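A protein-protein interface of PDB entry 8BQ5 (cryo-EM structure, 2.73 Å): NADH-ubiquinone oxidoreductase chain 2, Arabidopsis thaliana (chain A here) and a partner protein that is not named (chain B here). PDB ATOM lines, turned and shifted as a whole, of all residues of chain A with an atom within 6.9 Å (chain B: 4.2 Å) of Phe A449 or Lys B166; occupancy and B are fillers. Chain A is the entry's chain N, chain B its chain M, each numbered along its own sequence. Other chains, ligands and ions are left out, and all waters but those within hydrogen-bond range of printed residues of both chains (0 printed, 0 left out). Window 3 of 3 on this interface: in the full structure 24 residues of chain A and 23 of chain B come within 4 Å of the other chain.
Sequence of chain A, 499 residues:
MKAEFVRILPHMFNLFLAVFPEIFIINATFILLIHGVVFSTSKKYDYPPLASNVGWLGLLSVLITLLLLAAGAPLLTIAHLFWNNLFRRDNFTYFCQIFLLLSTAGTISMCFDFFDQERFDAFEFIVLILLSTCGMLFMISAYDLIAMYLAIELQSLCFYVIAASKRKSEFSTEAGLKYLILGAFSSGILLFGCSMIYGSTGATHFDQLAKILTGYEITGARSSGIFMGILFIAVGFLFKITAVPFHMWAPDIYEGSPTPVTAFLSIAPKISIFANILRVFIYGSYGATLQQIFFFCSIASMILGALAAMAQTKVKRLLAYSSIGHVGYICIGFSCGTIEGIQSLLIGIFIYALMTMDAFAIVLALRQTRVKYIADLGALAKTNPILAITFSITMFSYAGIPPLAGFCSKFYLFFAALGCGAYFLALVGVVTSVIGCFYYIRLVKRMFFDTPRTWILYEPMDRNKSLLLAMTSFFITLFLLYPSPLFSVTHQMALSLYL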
ATOM      1  N   ALA A 379       1.661   5.761 -28.094  1.00  0.00           N
ATOM      2  CA  ALA A 379       1.637   6.097 -29.517  1.00  0.00           C
ATOM      3  C   ALA A 379       1.197   4.931 -30.398  1.00  0.00           C
ATOM      4  O   ALA A 379       1.544   4.883 -31.580  1.00  0.00           O
ATOM      5  CB  ALA A 379       2.996   6.624 -29.990  1.00  0.00           C
ATOM      6  N   ALA A 381      -1.869   4.407 -31.315  1.00  0.00           N
ATOM      7  CA  ALA A 381      -2.834   4.971 -32.250  1.00  0.00           C
ATOM      8  C   ALA A 381      -2.162   5.564 -33.479  1.00  0.00           C
ATOM      9  O   ALA A 381      -2.827   5.771 -34.498  1.00  0.00           O
ATOM     10  CB  ALA A 381      -3.686   6.034 -31.556  1.00  0.00           C
ATOM     11  N   ILE A 441     -10.126   2.849 -19.246  1.00  0.00           N
ATOM     12  CA  ILE A 441      -9.878   3.977 -20.140  1.00  0.00           C
ATOM     13  C   ILE A 441      -8.486   4.558 -19.964  1.00  0.00           C
ATOM     14  O   ILE A 441      -8.040   5.332 -20.820  1.00  0.00           O
ATOM     15  CB  ILE A 441     -10.925   5.094 -19.966  1.00  0.00           C
ATOM     16  CG1 ILE A 441     -10.781   5.777 -18.607  1.00  0.00           C
ATOM     17  CG2 ILE A 441     -12.331   4.548 -20.158  1.00  0.00           C
ATOM     18  CD1 ILE A 441     -11.624   7.021 -18.474  1.00  0.00           C
ATOM     19  N   VAL A 444      -6.801   3.365 -23.023  1.00  0.00           N
ATOM     20  CA  VAL A 444      -7.135   4.170 -24.194  1.00  0.00           C
ATOM     21  C   VAL A 444      -6.373   5.486 -24.162  1.00  0.00           C
ATOM     22  O   VAL A 444      -5.868   5.954 -25.189  1.00  0.00           O
ATOM     23  CB  VAL A 444      -8.654   4.399 -24.276  1.00  0.00           C
ATOM     24  CG1 VAL A 444      -8.997   5.199 -25.522  1.00  0.00           C
ATOM     25  CG2 VAL A 444      -9.389   3.073 -24.265  1.00  0.00           C
ATOM     26  N   LYS A 445      -6.281   6.101 -22.983  1.00  0.00           N
ATOM     27  CA  LYS A 445      -5.518   7.335 -22.840  1.00  0.00           C
ATOM     28  C   LYS A 445      -4.052   7.120 -23.200  1.00  0.00           C
ATOM     29  O   LYS A 445      -3.440   7.962 -23.867  1.00  0.00           O
ATOM     30  CB  LYS A 445      -5.651   7.868 -21.413  1.00  0.00           C
ATOM     31  CG  LYS A 445      -4.572   8.861 -21.006  1.00  0.00           C
ATOM     32  CD  LYS A 445      -3.460   8.190 -20.213  1.00  0.00           C
ATOM     33  CE  LYS A 445      -2.434   9.200 -19.744  1.00  0.00           C
ATOM     34  NZ  LYS A 445      -1.187   8.532 -19.286  1.00  0.00           N
ATOM     35  N   ARG A 446      -3.470   6.005 -22.752  1.00  0.00           N
ATOM     36  CA  ARG A 446      -2.085   5.706 -23.101  1.00  0.00           C
ATOM     37  C   ARG A 446      -1.919   5.540 -24.606  1.00  0.00           C
ATOM     38  O   ARG A 446      -0.938   6.017 -25.186  1.00  0.00           O
ATOM     39  CB  ARG A 446      -1.614   4.445 -22.376  1.00  0.00           C
ATOM     40  CG  ARG A 446      -0.160   4.092 -22.640  1.00  0.00           C
ATOM     41  CD  ARG A 446       0.772   5.161 -22.113  1.00  0.00           C
ATOM     42  NE  ARG A 446       0.823   5.163 -20.657  1.00  0.00           N
ATOM     43  CZ  ARG A 446       1.730   5.809 -19.940  1.00  0.00           C
ATOM     44  NH1 ARG A 446       2.660   6.556 -20.514  1.00  0.00           N
ATOM     45  NH2 ARG A 446       1.704   5.708 -18.615  1.00  0.00           N
ATOM     46  N   MET A 447      -2.855   4.898 -25.288  1.00  0.00           N
ATOM     47  CA  MET A 447      -2.634   4.639 -26.735  1.00  0.00           C
ATOM     48  C   MET A 447      -2.981   5.866 -27.573  1.00  0.00           C
ATOM     49  O   MET A 447      -2.443   5.973 -28.674  1.00  0.00           O
ATOM     50  CB  MET A 447      -3.510   3.488 -27.229  1.00  0.00           C
ATOM     51  CG  MET A 447      -3.098   2.135 -26.699  1.00  0.00           C
ATOM     52  SD  MET A 447      -4.161   0.838 -27.361  1.00  0.00           S
ATOM     53  CE  MET A 447      -5.708   1.223 -26.544  1.00  0.00           C
ATOM     54  N   PHE A 448      -3.824   6.758 -27.067  1.00  0.00           N
ATOM     55  CA  PHE A 448      -4.312   7.848 -27.900  1.00  0.00           C
ATOM     56  C   PHE A 448      -3.849   9.230 -27.473  1.00  0.00           C
ATOM     57  O   PHE A 448      -3.639  10.081 -28.338  1.00  0.00           O
ATOM     58  CB  PHE A 448      -5.848   7.847 -27.927  1.00  0.00           C
ATOM     59  CG  PHE A 448      -6.438   6.864 -28.887  1.00  0.00           C
ATOM     60  CD1 PHE A 448      -6.640   5.547 -28.513  1.00  0.00           C
ATOM     61  CD2 PHE A 448      -6.804   7.256 -30.161  1.00  0.00           C
ATOM     62  CE1 PHE A 448      -7.187   4.641 -29.394  1.00  0.00           C
ATOM     63  CE2 PHE A 448      -7.352   6.354 -31.045  1.00  0.00           C
ATOM     64  CZ  PHE A 448      -7.545   5.045 -30.661  1.00  0.00           C
ATOM     65  N   PHE A 449      -3.693   9.485 -26.176  1.00  0.00           N
ATOM     66  CA  PHE A 449      -3.477  10.847 -25.704  1.00  0.00           C
ATOM     67  C   PHE A 449      -2.018  11.163 -25.409  1.00  0.00           C
ATOM     68  O   PHE A 449      -1.614  12.323 -25.526  1.00  0.00           O
ATOM     69  CB  PHE A 449      -4.292  11.130 -24.432  1.00  0.00           C
ATOM     70  CG  PHE A 449      -5.752  10.753 -24.515  1.00  0.00           C
ATOM     71  CD1 PHE A 449      -6.376  10.505 -25.726  1.00  0.00           C
ATOM     72  CD2 PHE A 449      -6.506  10.672 -23.358  1.00  0.00           C
ATOM     73  CE1 PHE A 449      -7.709  10.159 -25.774  1.00  0.00           C
ATOM     74  CE2 PHE A 449      -7.835  10.331 -23.402  1.00  0.00           C
ATOM     75  CZ  PHE A 449      -8.440  10.077 -24.611  1.00  0.00           C
ATOM     76  N   ASP A 450      -1.224  10.171 -25.021  1.00  0.00           N
ATOM     77  CA  ASP A 450       0.143  10.428 -24.596  1.00  0.00           C
ATOM     78  C   ASP A 450       1.062  10.643 -25.792  1.00  0.00           C
ATOM     79  O   ASP A 450       0.817  10.146 -26.895  1.00  0.00           O
ATOM     80  CB  ASP A 450       0.662   9.276 -23.737  1.00  0.00           C
ATOM     81  CG  ASP A 450       0.239   9.397 -22.290  1.00  0.00           C
ATOM     82  OD1 ASP A 450       0.156  10.539 -21.788  1.00  0.00           O
ATOM     83  OD2 ASP A 450      -0.016   8.355 -21.654  1.00  0.00           O
ATOM     84  N   THR A 451       2.130  11.403 -25.559  1.00  0.00           N
ATOM     85  CA  THR A 451       3.139  11.706 -26.573  1.00  0.00           C
ATOM     86  C   THR A 451       4.504  11.392 -25.978  1.00  0.00           C
ATOM     87  O   THR A 451       5.245  12.300 -25.575  1.00  0.00           O
ATOM     88  CB  THR A 451       3.050  13.162 -27.035  1.00  0.00           C
ATOM     89  OG1 THR A 451       3.023  14.030 -25.895  1.00  0.00           O
ATOM     90  CG2 THR A 451       1.797  13.384 -27.864  1.00  0.00           C
ATOM     91  N   PRO A 452       4.868  10.115 -25.905  1.00  0.00           N
ATOM     92  CA  PRO A 452       6.132   9.741 -25.264  1.00  0.00           C
ATOM     93  C   PRO A 452       7.336  10.141 -26.102  1.00  0.00           C
ATOM     94  O   PRO A 452       7.267  10.284 -27.324  1.00  0.00           O
ATOM     95  CB  PRO A 452       6.039   8.216 -25.129  1.00  0.00           C
ATOM     96  CG  PRO A 452       4.857   7.788 -25.941  1.00  0.00           C
ATOM     97  CD  PRO A 452       4.222   8.980 -26.580  1.00  0.00           C
ATOM     98  N   PHE B 154     -14.722  11.516 -25.287  1.00  0.00           N
ATOM     99  CA  PHE B 154     -13.453  11.201 -24.644  1.00  0.00           C
ATOM    100  C   PHE B 154     -12.313  11.267 -25.647  1.00  0.00           C
ATOM    101  O   PHE B 154     -11.276  11.895 -25.395  1.00  0.00           O
ATOM    102  CB  PHE B 154     -13.561   9.805 -24.019  1.00  0.00           C
ATOM    103  CG  PHE B 154     -12.392   9.402 -23.167  1.00  0.00           C
ATOM    104  CD1 PHE B 154     -12.094  10.080 -22.000  1.00  0.00           C
ATOM    105  CD2 PHE B 154     -11.617   8.307 -23.514  1.00  0.00           C
ATOM    106  CE1 PHE B 154     -11.031   9.692 -21.210  1.00  0.00           C
ATOM    107  CE2 PHE B 154     -10.553   7.915 -22.730  1.00  0.00           C
ATOM    108  CZ  PHE B 154     -10.259   8.607 -21.577  1.00  0.00           C
ATOM    109  N   ILE B 157     -11.688  14.977 -26.844  1.00  0.00           N
ATOM    110  CA  ILE B 157     -10.972  15.782 -25.859  1.00  0.00           C
ATOM    111  C   ILE B 157      -9.515  15.345 -25.765  1.00  0.00           C
ATOM    112  O   ILE B 157      -8.600  16.176 -25.794  1.00  0.00           O
ATOM    113  CB  ILE B 157     -11.658  15.708 -24.483  1.00  0.00           C
ATOM    114  CG1 ILE B 157     -13.015  16.401 -24.514  1.00  0.00           C
ATOM    115  CG2 ILE B 157     -10.775  16.347 -23.426  1.00  0.00           C
ATOM    116  CD1 ILE B 157     -13.893  16.049 -23.334  1.00  0.00           C
ATOM    117  N   GLY B 158      -9.275  14.037 -25.650  1.00  0.00           N
ATOM    118  CA  GLY B 158      -7.933  13.574 -25.349  1.00  0.00           C
ATOM    119  C   GLY B 158      -6.970  13.701 -26.513  1.00  0.00           C
ATOM    120  O   GLY B 158      -5.780  13.960 -26.315  1.00  0.00           O
ATOM    121  N   VAL B 159      -7.458  13.488 -27.736  1.00  0.00           N
ATOM    122  CA  VAL B 159      -6.535  13.489 -28.911  1.00  0.00           C
ATOM    123  C   VAL B 159      -6.305  14.917 -29.420  1.00  0.00           C
ATOM    124  O   VAL B 159      -5.132  15.275 -29.602  1.00  0.00           O
ATOM    125  CB  VAL B 159      -7.022  12.554 -30.037  1.00  0.00           C
ATOM    126  CG1 VAL B 159      -6.143  12.637 -31.274  1.00  0.00           C
ATOM    127  CG2 VAL B 159      -7.142  11.114 -29.566  1.00  0.00           C
ATOM    128  N   GLY B 161      -7.221  17.891 -27.951  1.00  0.00           N
ATOM    129  CA  GLY B 161      -7.107  18.949 -26.931  1.00  0.00           C
ATOM    130  C   GLY B 161      -5.769  19.650 -27.069  1.00  0.00           C
ATOM    131  O   GLY B 161      -4.864  19.068 -27.688  1.00  0.00           O
ATOM    132  N   ARG B 163      -3.450  21.149 -24.474  1.00  0.00           N
ATOM    133  CA  ARG B 163      -2.338  20.938 -23.511  1.00  0.00           C
ATOM    134  C   ARG B 163      -2.417  19.564 -22.851  1.00  0.00           C
ATOM    135  O   ARG B 163      -3.351  18.830 -23.157  1.00  0.00           O
ATOM    136  CB  ARG B 163      -2.421  22.022 -22.435  1.00  0.00           C
ATOM    137  CG  ARG B 163      -2.403  23.444 -22.974  1.00  0.00           C
ATOM    138  CD  ARG B 163      -2.410  24.450 -21.842  1.00  0.00           C
ATOM    139  NE  ARG B 163      -3.600  24.342 -21.012  1.00  0.00           N
ATOM    140  CZ  ARG B 163      -3.823  25.060 -19.919  1.00  0.00           C
ATOM    141  NH1 ARG B 163      -4.939  24.891 -19.234  1.00  0.00           N
ATOM    142  NH2 ARG B 163      -2.928  25.941 -19.511  1.00  0.00           N
ATOM    143  N   GLN B 164      -1.493  19.264 -21.933  1.00  0.00           N
ATOM    144  CA  GLN B 164      -1.531  18.004 -21.203  1.00  0.00           C
ATOM    145  C   GLN B 164      -2.582  17.973 -20.101  1.00  0.00           C
ATOM    146  O   GLN B 164      -2.820  16.901 -19.534  1.00  0.00           O
ATOM    147  CB  GLN B 164      -0.148  17.709 -20.621  1.00  0.00           C
ATOM    148  CG  GLN B 164       0.687  16.787 -21.493  1.00  0.00           C
ATOM    149  CD  GLN B 164       1.360  17.512 -22.646  1.00  0.00           C
ATOM    150  OE1 GLN B 164       0.969  18.620 -23.019  1.00  0.00           O
ATOM    151  NE2 GLN B 164       2.379  16.883 -23.221  1.00  0.00           N
ATOM    152  N   ARG B 165      -3.212  19.106 -19.783  1.00  0.00           N
ATOM    153  CA  ARG B 165      -4.335  19.098 -18.851  1.00  0.00           C
ATOM    154  C   ARG B 165      -5.534  18.342 -19.416  1.00  0.00           C
ATOM    155  O   ARG B 165      -6.463  18.011 -18.663  1.00  0.00           O
ATOM    156  CB  ARG B 165      -4.730  20.534 -18.505  1.00  0.00           C
ATOM    157  CG  ARG B 165      -3.726  21.275 -17.630  1.00  0.00           C
ATOM    158  CD  ARG B 165      -4.354  22.494 -16.959  1.00  0.00           C
ATOM    159  NE  ARG B 165      -5.174  22.160 -15.801  1.00  0.00           N
ATOM    160  CZ  ARG B 165      -4.694  21.745 -14.635  1.00  0.00           C
ATOM    161  NH1 ARG B 165      -3.395  21.593 -14.436  1.00  0.00           N
ATOM    162  NH2 ARG B 165      -5.540  21.485 -13.642  1.00  0.00           N
ATOM    163  N   LYS B 166      -5.525  18.066 -20.725  1.00  0.00           N
ATOM    164  CA  LYS B 166      -6.621  17.335 -21.348  1.00  0.00           C
ATOM    165  C   LYS B 166      -6.774  15.936 -20.765  1.00  0.00           C
ATOM    166  O   LYS B 166      -7.880  15.392 -20.766  1.00  0.00           O
ATOM    167  CB  LYS B 166      -6.420  17.262 -22.865  1.00  0.00           C
ATOM    168  CG  LYS B 166      -5.321  16.309 -23.313  1.00  0.00           C
ATOM    169  CD  LYS B 166      -4.792  16.660 -24.695  1.00  0.00           C
ATOM    170  CE  LYS B 166      -3.534  15.869 -25.013  1.00  0.00           C
ATOM    171  NZ  LYS B 166      -3.449  15.464 -26.440  1.00  0.00           N
ATOM    172  N   ILE B 167      -5.691  15.348 -20.252  1.00  0.00           N
ATOM    173  CA  ILE B 167      -5.778  14.030 -19.621  1.00  0.00           C
ATOM    174  C   ILE B 167      -6.734  14.076 -18.436  1.00  0.00           C
ATOM    175  O   ILE B 167      -7.731  13.342 -18.379  1.00  0.00           O
ATOM    176  CB  ILE B 167      -4.384  13.550 -19.178  1.00  0.00           C
ATOM    177  CG1 ILE B 167      -3.352  13.764 -20.286  1.00  0.00           C
ATOM    178  CG2 ILE B 167      -4.430  12.092 -18.757  1.00  0.00           C
ATOM    179  CD1 ILE B 167      -3.509  12.829 -21.441  1.00  0.00           C
ATOM    180  N   LYS B 168      -6.429  14.944 -17.470  1.00  0.00           N
ATOM    181  CA  LYS B 168      -7.280  15.109 -16.300  1.00  0.00           C
ATOM    182  C   LYS B 168      -8.688  15.521 -16.703  1.00  0.00           C
ATOM    183  O   LYS B 168      -9.674  15.031 -16.135  1.00  0.00           O
ATOM    184  CB  LYS B 168      -6.660  16.147 -15.363  1.00  0.00           C
ATOM    185  CG  LYS B 168      -7.100  16.062 -13.914  1.00  0.00           C
ATOM    186  CD  LYS B 168      -6.844  17.382 -13.208  1.00  0.00           C
ATOM    187  CE  LYS B 168      -7.380  17.373 -11.789  1.00  0.00           C
ATOM    188  NZ  LYS B 168      -6.625  18.304 -10.913  1.00  0.00           N
ATOM    189  N   ALA B 169      -8.801  16.414 -17.690  1.00  0.00           N
ATOM    190  CA  ALA B 169     -10.117  16.897 -18.100  1.00  0.00           C
ATOM    191  C   ALA B 169     -10.984  15.763 -18.643  1.00  0.00           C
ATOM    192  O   ALA B 169     -12.150  15.614 -18.256  1.00  0.00           O
ATOM    193  CB  ALA B 169      -9.960  18.006 -19.138  1.00  0.00           C
ATOM    194  N   ALA B 170     -10.424  14.946 -19.539  1.00  0.00           N
ATOM    195  CA  ALA B 170     -11.170  13.833 -20.113  1.00  0.00           C
ATOM    196  C   ALA B 170     -11.520  12.795 -19.054  1.00  0.00           C
ATOM    197  O   ALA B 170     -12.630  12.243 -19.061  1.00  0.00           O
ATOM    198  CB  ALA B 170     -10.370  13.202 -21.251  1.00  0.00           C
ATOM    199  N   GLU B 243     -10.375  22.499 -21.818  1.00  0.00           N
ATOM    200  CA  GLU B 243      -9.284  21.701 -22.371  1.00  0.00           C
ATOM    201  C   GLU B 243      -9.623  21.086 -23.724  1.00  0.00           C
ATOM    202  O   GLU B 243      -8.711  20.677 -24.450  1.00  0.00           O
ATOM    203  CB  GLU B 243      -8.892  20.592 -21.393  1.00  0.00           C
ATOM    204  CG  GLU B 243      -8.028  21.047 -20.226  1.00  0.00           C
ATOM    205  CD  GLU B 243      -7.136  22.228 -20.565  1.00  0.00           C
ATOM    206  OE1 GLU B 243      -6.223  22.067 -21.402  1.00  0.00           O
ATOM    207  OE2 GLU B 243      -7.340  23.314 -19.987  1.00  0.00           O
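Of the printed residues of chain B, Ile A441 touches Phe B154.
Of chain B, only Phe B154 (3.5 Å), Gly B158 (3.3 Å), Val B159 (3.8 Å), Lys B166 (3.8 Å) and Ile B167 (3.5 Å) come within 4 Å of Phe A449.
Asp A450 touches none of the printed residues of chain B.
Printed residues of chain A within 4 Å of Phe B154: Ile A441 and Phe A449.
Of the printed residues of chain A, Ile B167 touches Lys A445 and Phe A449.
The nearest printed residue of chain B that does not touch Phe A449 is Ala B170 (4.4 Å).
The nearest residue of chain A that does not touch Lys B166 is Phe A448 (5.7 Å).
The nearest printed residue of chain B that does not touch Phe A448 is Gly B158 (4.9 Å).
Of the 14 printed residues of chain B, 6 touch a printed residue of chain A.
Among the printed residues, no Asp or Glu carboxylate lies within 4 Å of a Lys or Arg side-chain nitrogen of the other chain.
Among the printed residues, merely in contact across the chains: Ile A441 with Phe B154 (3.7 Å), Lys A445 with Ile B167 (3.6 Å), Phe A448 with Val B159 (3.9 Å), Phe A449 with Phe B154 (3.5 Å), Phe A449 with Gly B158 (3.3 Å), Phe A449 with Val B159 (3.8 Å), Phe A449 with Lys B166 (3.8 Å), Phe A449 with Ile B167 (3.5 Å) and Thr A451 with Gln B164 (3.96 Å).
The backbone carbonyl oxygen (O) of Gly B158 sits at hydrogen-bond distance from the side-chain amino group (NZ) of Lys B166, at 2.8 Å.
The side-chain amino group (NZ) of Lys A445 lies within salt-bridge range of the side-chain carboxylate (OD2) of Asp A450 (2.6 Å).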
